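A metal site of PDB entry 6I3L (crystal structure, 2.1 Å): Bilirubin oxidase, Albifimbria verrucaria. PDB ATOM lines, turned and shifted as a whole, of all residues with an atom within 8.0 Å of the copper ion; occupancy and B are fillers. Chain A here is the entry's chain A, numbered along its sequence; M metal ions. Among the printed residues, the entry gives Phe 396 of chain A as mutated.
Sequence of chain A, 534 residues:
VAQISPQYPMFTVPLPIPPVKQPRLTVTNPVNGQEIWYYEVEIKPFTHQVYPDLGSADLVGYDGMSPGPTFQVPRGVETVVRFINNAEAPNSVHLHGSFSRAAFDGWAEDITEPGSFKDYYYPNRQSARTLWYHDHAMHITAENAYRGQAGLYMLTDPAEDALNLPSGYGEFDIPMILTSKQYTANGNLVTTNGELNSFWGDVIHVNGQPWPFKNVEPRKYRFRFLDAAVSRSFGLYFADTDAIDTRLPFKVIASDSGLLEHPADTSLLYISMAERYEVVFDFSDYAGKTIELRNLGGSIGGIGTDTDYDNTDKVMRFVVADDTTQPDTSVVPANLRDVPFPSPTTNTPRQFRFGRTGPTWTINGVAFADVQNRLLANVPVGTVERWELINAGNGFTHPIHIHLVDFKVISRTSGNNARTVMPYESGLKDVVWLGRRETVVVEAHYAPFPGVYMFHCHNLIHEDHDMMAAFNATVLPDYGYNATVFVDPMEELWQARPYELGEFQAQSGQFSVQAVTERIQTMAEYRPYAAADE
The copper ion is bound by ND1 of His 398 (1.9 Å).
A ring nitrogen (ND1) of His 462 is bound to the copper ion (2.0 Å).
SG of Cys 457 binds the copper ion (2.2 Å).
ND1 of His 398 lies close to SD of Met 467, at 3.4 Å.
The backbone carbonyl oxygen (O) of Met 467 is in hydrogen-bond range of the backbone NH (N) of Cys 457 (3.2 Å).
N of Met 467 sits at hydrogen-bond distance from O of Trp 361 (3.2 Å).
O of His 398 is in hydrogen-bond range of N of Leu 434 (3.0 Å).
The backbone carbonyl oxygen (O) of His 462 lies within hydrogen-bond range of the backbone NH (N) of Met 467 (2.9 Å).
The side-chain hydroxyl of Thr 397 is in hydrogen-bond range of the indole nitrogen of Trp 433, 3.0 Å away.
SG of Cys 457 sits close to N of Asn 459, 3.3 Å away.
The backbone carbonyl oxygen (O) of Asn 197 lies within hydrogen-bond range of a ring nitrogen (NE2) of His 462, at 2.9 Å.
Residues that only touch the copper ion: Thr 397 (3.5 Å) and Met 467 (3.4 Å).
Five residues have an atom within 4 Å of the copper ion: Thr 397, His 398, Cys 457, His 462 and Met 467.
The nearest printed residue that does not touch the copper ion is Asn 459 (4.01 Å).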
ATOM      1  N   ASN A 197      17.889  24.271   5.416  1.00  0.00           N
ATOM      2  CA  ASN A 197      19.015  23.752   6.237  1.00  0.00           C
ATOM      3  C   ASN A 197      19.676  24.938   6.961  1.00  0.00           C
ATOM      4  O   ASN A 197      19.527  25.048   8.183  1.00  0.00           O
ATOM      5  CB  ASN A 197      19.954  22.874   5.394  1.00  0.00           C
ATOM      6  CG  ASN A 197      19.246  21.618   4.912  1.00  0.00           C
ATOM      7  OD1 ASN A 197      18.447  21.018   5.635  1.00  0.00           O
ATOM      8  ND2 ASN A 197      19.475  21.237   3.666  1.00  0.00           N
ATOM      9  N   SER A 198      20.340  25.819   6.219  1.00  0.00           N
ATOM     10  CA  SER A 198      21.048  27.017   6.750  1.00  0.00           C
ATOM     11  C   SER A 198      21.345  27.919   5.569  1.00  0.00           C
ATOM     12  O   SER A 198      21.647  27.381   4.477  1.00  0.00           O
ATOM     13  CB  SER A 198      22.329  26.659   7.502  1.00  0.00           C
ATOM     14  OG  SER A 198      22.088  26.337   8.870  1.00  0.00           O
ATOM     15  N   MET A 273      24.719  33.251  16.298  1.00  0.00           N
ATOM     16  CA  MET A 273      23.565  34.115  15.969  1.00  0.00           C
ATOM     17  C   MET A 273      22.918  34.620  17.280  1.00  0.00           C
ATOM     18  O   MET A 273      22.666  33.812  18.173  1.00  0.00           O
ATOM     19  CB  MET A 273      22.557  33.370  15.106  1.00  0.00           C
ATOM     20  CG  MET A 273      23.055  33.126  13.678  1.00  0.00           C
ATOM     21  SD  MET A 273      24.294  31.801  13.500  1.00  0.00           S
ATOM     22  CE  MET A 273      23.261  30.354  13.637  1.00  0.00           C
ATOM     23  N   PHE A 354      17.678  19.212  20.578  1.00  0.00           N
ATOM     24  CA  PHE A 354      17.590  20.053  19.379  1.00  0.00           C
ATOM     25  C   PHE A 354      18.025  19.215  18.189  1.00  0.00           C
ATOM     26  O   PHE A 354      19.219  18.963  18.047  1.00  0.00           O
ATOM     27  CB  PHE A 354      18.424  21.323  19.584  1.00  0.00           C
ATOM     28  CG  PHE A 354      17.894  22.161  20.713  1.00  0.00           C
ATOM     29  CD1 PHE A 354      18.265  21.900  22.031  1.00  0.00           C
ATOM     30  CD2 PHE A 354      16.944  23.141  20.469  1.00  0.00           C
ATOM     31  CE1 PHE A 354      17.730  22.647  23.073  1.00  0.00           C
ATOM     32  CE2 PHE A 354      16.406  23.867  21.521  1.00  0.00           C
ATOM     33  CZ  PHE A 354      16.819  23.629  22.816  1.00  0.00           C
ATOM     34  N   GLY A 355      17.063  18.749  17.401  1.00  0.00           N
ATOM     35  CA  GLY A 355      17.342  17.833  16.302  1.00  0.00           C
ATOM     36  C   GLY A 355      16.337  18.016  15.184  1.00  0.00           C
ATOM     37  O   GLY A 355      15.783  19.103  15.069  1.00  0.00           O
ATOM     38  N   TRP A 361      13.077  20.975  11.726  1.00  0.00           N
ATOM     39  CA  TRP A 361      13.872  21.261  12.958  1.00  0.00           C
ATOM     40  C   TRP A 361      12.929  21.347  14.179  1.00  0.00           C
ATOM     41  O   TRP A 361      11.949  22.127  14.109  1.00  0.00           O
ATOM     42  CB  TRP A 361      14.680  22.532  12.756  1.00  0.00           C
ATOM     43  CG  TRP A 361      15.599  22.453  11.579  1.00  0.00           C
ATOM     44  CD1 TRP A 361      15.397  23.007  10.341  1.00  0.00           C
ATOM     45  CD2 TRP A 361      16.872  21.795  11.513  1.00  0.00           C
ATOM     46  NE1 TRP A 361      16.455  22.745   9.522  1.00  0.00           N
ATOM     47  CE2 TRP A 361      17.389  22.011  10.219  1.00  0.00           C
ATOM     48  CE3 TRP A 361      17.658  21.095  12.437  1.00  0.00           C
ATOM     49  CZ2 TRP A 361      18.642  21.541   9.817  1.00  0.00           C
ATOM     50  CZ3 TRP A 361      18.895  20.621  12.041  1.00  0.00           C
ATOM     51  CH2 TRP A 361      19.360  20.824  10.748  1.00  0.00           C
ATOM     52  N   THR A 362      13.241  20.610  15.250  1.00  0.00           N
ATOM     53  CA  THR A 362      12.314  20.358  16.368  1.00  0.00           C
ATOM     54  C   THR A 362      13.038  20.446  17.705  1.00  0.00           C
ATOM     55  O   THR A 362      14.248  20.341  17.768  1.00  0.00           O
ATOM     56  CB  THR A 362      11.657  18.974  16.252  1.00  0.00           C
ATOM     57  OG1 THR A 362      12.663  17.972  16.111  1.00  0.00           O
ATOM     58  CG2 THR A 362      10.711  18.884  15.079  1.00  0.00           C
ATOM     59  N   ASN A 391      22.530  19.147  21.763  1.00  0.00           N
ATOM     60  CA  ASN A 391      22.702  18.941  20.304  1.00  0.00           C
ATOM     61  C   ASN A 391      23.344  17.563  20.149  1.00  0.00           C
ATOM     62  O   ASN A 391      24.548  17.445  20.416  1.00  0.00           O
ATOM     63  CB  ASN A 391      23.562  20.046  19.670  1.00  0.00           C
ATOM     64  CG  ASN A 391      23.738  19.820  18.189  1.00  0.00           C
ATOM     65  OD1 ASN A 391      22.994  19.022  17.614  1.00  0.00           O
ATOM     66  ND2 ASN A 391      24.727  20.478  17.597  1.00  0.00           N
ATOM     67  N   PHE A 396      25.053  19.688  12.344  1.00  0.00           N
ATOM     68  CA  PHE A 396      24.445  21.041  12.506  1.00  0.00           C
ATOM     69  C   PHE A 396      24.779  21.593  13.894  1.00  0.00           C
ATOM     70  O   PHE A 396      25.140  20.775  14.778  1.00  0.00           O
ATOM     71  CB  PHE A 396      22.947  20.965  12.241  1.00  0.00           C
ATOM     72  CG  PHE A 396      22.259  19.735  12.804  1.00  0.00           C
ATOM     73  CD1 PHE A 396      22.041  19.592  14.172  1.00  0.00           C
ATOM     74  CD2 PHE A 396      21.802  18.719  11.960  1.00  0.00           C
ATOM     75  CE1 PHE A 396      21.413  18.475  14.685  1.00  0.00           C
ATOM     76  CE2 PHE A 396      21.180  17.591  12.479  1.00  0.00           C
ATOM     77  CZ  PHE A 396      20.960  17.481  13.830  1.00  0.00           C
ATOM     78  N   THR A 397      24.664  22.914  14.086  1.00  0.00           N
ATOM     79  CA  THR A 397      24.794  23.602  15.413  1.00  0.00           C
ATOM     80  C   THR A 397      23.627  24.558  15.674  1.00  0.00           C
ATOM     81  O   THR A 397      22.978  24.989  14.731  1.00  0.00           O
ATOM     82  CB  THR A 397      26.109  24.356  15.574  1.00  0.00           C
ATOM     83  OG1 THR A 397      26.103  25.502  14.732  1.00  0.00           O
ATOM     84  CG2 THR A 397      27.305  23.475  15.268  1.00  0.00           C
ATOM     85  N   HIS A 398      23.426  24.904  16.944  1.00  0.00           N
ATOM     86  CA  HIS A 398      22.199  25.596  17.430  1.00  0.00           C
ATOM     87  C   HIS A 398      22.570  26.591  18.510  1.00  0.00           C
ATOM     88  O   HIS A 398      22.845  26.198  19.623  1.00  0.00           O
ATOM     89  CB  HIS A 398      21.173  24.583  17.989  1.00  0.00           C
ATOM     90  CG  HIS A 398      20.900  23.463  17.053  1.00  0.00           C
ATOM     91  ND1 HIS A 398      20.201  23.652  15.878  1.00  0.00           N
ATOM     92  CD2 HIS A 398      21.216  22.149  17.117  1.00  0.00           C
ATOM     93  CE1 HIS A 398      20.119  22.481  15.258  1.00  0.00           C
ATOM     94  NE2 HIS A 398      20.719  21.556  16.005  1.00  0.00           N
ATOM     95  N   PRO A 399      22.586  27.909  18.218  1.00  0.00           N
ATOM     96  CA  PRO A 399      22.596  28.920  19.259  1.00  0.00           C
ATOM     97  C   PRO A 399      21.183  29.021  19.858  1.00  0.00           C
ATOM     98  O   PRO A 399      20.256  29.491  19.203  1.00  0.00           O
ATOM     99  CB  PRO A 399      23.068  30.169  18.508  1.00  0.00           C
ATOM    100  CG  PRO A 399      22.480  29.994  17.159  1.00  0.00           C
ATOM    101  CD  PRO A 399      22.572  28.503  16.876  1.00  0.00           C
ATOM    102  N   ILE A 400      21.060  28.572  21.103  1.00  0.00           N
ATOM    103  CA  ILE A 400      19.774  28.462  21.830  1.00  0.00           C
ATOM    104  C   ILE A 400      19.533  29.719  22.659  1.00  0.00           C
ATOM    105  O   ILE A 400      20.392  30.126  23.469  1.00  0.00           O
ATOM    106  CB  ILE A 400      19.739  27.200  22.701  1.00  0.00           C
ATOM    107  CG1 ILE A 400      19.982  25.927  21.887  1.00  0.00           C
ATOM    108  CG2 ILE A 400      18.432  27.148  23.466  1.00  0.00           C
ATOM    109  CD1 ILE A 400      18.991  25.692  20.785  1.00  0.00           C
ATOM    110  N   TRP A 433      25.757  28.827  22.391  1.00  0.00           N
ATOM    111  CA  TRP A 433      26.033  28.033  21.171  1.00  0.00           C
ATOM    112  C   TRP A 433      26.288  26.561  21.520  1.00  0.00           C
ATOM    113  O   TRP A 433      27.305  26.270  22.228  1.00  0.00           O
ATOM    114  CB  TRP A 433      27.192  28.637  20.406  1.00  0.00           C
ATOM    115  CG  TRP A 433      27.380  28.106  19.028  1.00  0.00           C
ATOM    116  CD1 TRP A 433      26.467  27.462  18.247  1.00  0.00           C
ATOM    117  CD2 TRP A 433      28.563  28.244  18.220  1.00  0.00           C
ATOM    118  NE1 TRP A 433      26.995  27.185  17.020  1.00  0.00           N
ATOM    119  CE2 TRP A 433      28.282  27.656  16.968  1.00  0.00           C
ATOM    120  CE3 TRP A 433      29.835  28.764  18.450  1.00  0.00           C
ATOM    121  CZ2 TRP A 433      29.235  27.574  15.951  1.00  0.00           C
ATOM    122  CZ3 TRP A 433      30.766  28.701  17.439  1.00  0.00           C
ATOM    123  CH2 TRP A 433      30.473  28.110  16.205  1.00  0.00           C
ATOM    124  N   LEU A 434      25.383  25.693  21.051  1.00  0.00           N
ATOM    125  CA  LEU A 434      25.579  24.225  21.009  1.00  0.00           C
ATOM    126  C   LEU A 434      26.307  23.919  19.701  1.00  0.00           C
ATOM    127  O   LEU A 434      25.636  23.808  18.684  1.00  0.00           O
ATOM    128  CB  LEU A 434      24.244  23.471  21.055  1.00  0.00           C
ATOM    129  CG  LEU A 434      23.280  23.888  22.151  1.00  0.00           C
ATOM    130  CD1 LEU A 434      22.016  23.013  22.088  1.00  0.00           C
ATOM    131  CD2 LEU A 434      23.922  23.782  23.521  1.00  0.00           C
ATOM    132  N   HIS A 456      14.145  28.836  21.671  1.00  0.00           N
ATOM    133  CA  HIS A 456      14.381  28.360  20.289  1.00  0.00           C
ATOM    134  C   HIS A 456      15.858  28.450  19.944  1.00  0.00           C
ATOM    135  O   HIS A 456      16.660  29.162  20.628  1.00  0.00           O
ATOM    136  CB  HIS A 456      13.553  29.171  19.288  1.00  0.00           C
ATOM    137  CG  HIS A 456      13.792  30.637  19.338  1.00  0.00           C
ATOM    138  ND1 HIS A 456      14.686  31.282  18.502  1.00  0.00           N
ATOM    139  CD2 HIS A 456      13.254  31.598  20.134  1.00  0.00           C
ATOM    140  CE1 HIS A 456      14.683  32.573  18.766  1.00  0.00           C
ATOM    141  NE2 HIS A 456      13.805  32.789  19.772  1.00  0.00           N
ATOM    142  N   CYS A 457      16.170  27.788  18.844  1.00  0.00           N
ATOM    143  CA  CYS A 457      17.415  28.010  18.099  1.00  0.00           C
ATOM    144  C   CYS A 457      17.311  29.367  17.373  1.00  0.00           C
ATOM    145  O   CYS A 457      16.235  29.631  16.811  1.00  0.00           O
ATOM    146  CB  CYS A 457      17.653  26.857  17.151  1.00  0.00           C
ATOM    147  SG  CYS A 457      19.119  27.148  16.162  1.00  0.00           S
ATOM    148  N   HIS A 458      18.391  30.173  17.371  1.00  0.00           N
ATOM    149  CA  HIS A 458      18.466  31.480  16.677  1.00  0.00           C
ATOM    150  C   HIS A 458      19.183  31.399  15.339  1.00  0.00           C
ATOM    151  O   HIS A 458      19.418  32.511  14.730  1.00  0.00           O
ATOM    152  CB  HIS A 458      19.124  32.539  17.575  1.00  0.00           C
ATOM    153  CG  HIS A 458      18.482  33.891  17.480  1.00  0.00           C
ATOM    154  ND1 HIS A 458      18.628  34.683  16.362  1.00  0.00           N
ATOM    155  CD2 HIS A 458      17.770  34.613  18.378  1.00  0.00           C
ATOM    156  CE1 HIS A 458      17.987  35.821  16.559  1.00  0.00           C
ATOM    157  NE2 HIS A 458      17.471  35.820  17.799  1.00  0.00           N
ATOM    158  N   ASN A 459      19.527  30.199  14.851  1.00  0.00           N
ATOM    159  CA  ASN A 459      19.668  29.993  13.373  1.00  0.00           C
ATOM    160  C   ASN A 459      18.277  30.230  12.782  1.00  0.00           C
ATOM    161  O   ASN A 459      17.368  29.410  13.045  1.00  0.00           O
ATOM    162  CB  ASN A 459      20.223  28.605  13.000  1.00  0.00           C
ATOM    163  CG  ASN A 459      20.476  28.436  11.514  1.00  0.00           C
ATOM    164  OD1 ASN A 459      19.726  28.956  10.675  1.00  0.00           O
ATOM    165  ND2 ASN A 459      21.541  27.727  11.152  1.00  0.00           N
ATOM    166  N   LEU A 460      18.080  31.327  12.062  1.00  0.00           N
ATOM    167  CA  LEU A 460      16.694  31.760  11.736  1.00  0.00           C
ATOM    168  C   LEU A 460      16.063  30.750  10.766  1.00  0.00           C
ATOM    169  O   LEU A 460      14.822  30.635  10.759  1.00  0.00           O
ATOM    170  CB  LEU A 460      16.691  33.195  11.210  1.00  0.00           C
ATOM    171  CG  LEU A 460      17.227  34.249  12.191  1.00  0.00           C
ATOM    172  CD1 LEU A 460      17.227  35.625  11.550  1.00  0.00           C
ATOM    173  CD2 LEU A 460      16.443  34.279  13.494  1.00  0.00           C
ATOM    174  N   ILE A 461      16.857  30.007  10.007  1.00  0.00           N
ATOM    175  CA  ILE A 461      16.319  28.962   9.101  1.00  0.00           C
ATOM    176  C   ILE A 461      15.759  27.842   9.972  1.00  0.00           C
ATOM    177  O   ILE A 461      14.640  27.379   9.720  1.00  0.00           O
ATOM    178  CB  ILE A 461      17.392  28.451   8.135  1.00  0.00           C
ATOM    179  CG1 ILE A 461      17.881  29.539   7.192  1.00  0.00           C
ATOM    180  CG2 ILE A 461      16.884  27.212   7.399  1.00  0.00           C
ATOM    181  CD1 ILE A 461      16.796  30.115   6.273  1.00  0.00           C
ATOM    182  N   HIS A 462      16.481  27.439  11.009  1.00  0.00           N
ATOM    183  CA  HIS A 462      16.011  26.368  11.908  1.00  0.00           C
ATOM    184  C   HIS A 462      14.759  26.845  12.642  1.00  0.00           C
ATOM    185  O   HIS A 462      13.772  26.092  12.722  1.00  0.00           O
ATOM    186  CB  HIS A 462      17.084  25.929  12.900  1.00  0.00           C
ATOM    187  CG  HIS A 462      18.304  25.339  12.282  1.00  0.00           C
ATOM    188  ND1 HIS A 462      19.390  24.957  13.051  1.00  0.00           N
ATOM    189  CD2 HIS A 462      18.630  25.093  10.995  1.00  0.00           C
ATOM    190  CE1 HIS A 462      20.332  24.514  12.253  1.00  0.00           C
ATOM    191  NE2 HIS A 462      19.881  24.565  10.984  1.00  0.00           N
ATOM    192  N   GLU A 463      14.819  28.052  13.206  1.00  0.00           N
ATOM    193  CA  GLU A 463      13.699  28.672  13.962  1.00  0.00           C
ATOM    194  C   GLU A 463      12.411  28.664  13.108  1.00  0.00           C
ATOM    195  O   GLU A 463      11.355  28.326  13.650  1.00  0.00           O
ATOM    196  CB  GLU A 463      14.091  30.103  14.339  1.00  0.00           C
ATOM    197  CG  GLU A 463      13.088  30.805  15.231  1.00  0.00           C
ATOM    198  CD  GLU A 463      13.435  32.266  15.472  1.00  0.00           C
ATOM    199  OE1 GLU A 463      14.663  32.571  15.570  1.00  0.00           O
ATOM    200  OE2 GLU A 463      12.484  33.083  15.560  1.00  0.00           O
ATOM    201  N   MET A 467      12.093  25.271  14.887  1.00  0.00           N
ATOM    202  CA  MET A 467      12.809  24.786  16.088  1.00  0.00           C
ATOM    203  C   MET A 467      12.593  25.793  17.220  1.00  0.00           C
ATOM    204  O   MET A 467      13.522  26.554  17.564  1.00  0.00           O
ATOM    205  CB  MET A 467      14.313  24.647  15.798  1.00  0.00           C
ATOM    206  CG  MET A 467      15.108  24.022  16.943  1.00  0.00           C
ATOM    207  SD  MET A 467      16.824  23.696  16.463  1.00  0.00           S
ATOM    208  CE  MET A 467      16.723  21.953  16.082  1.00  0.00           C
HETATM  209 CU    CU M   1      19.506  25.240  15.053  1.00  0.00          CU
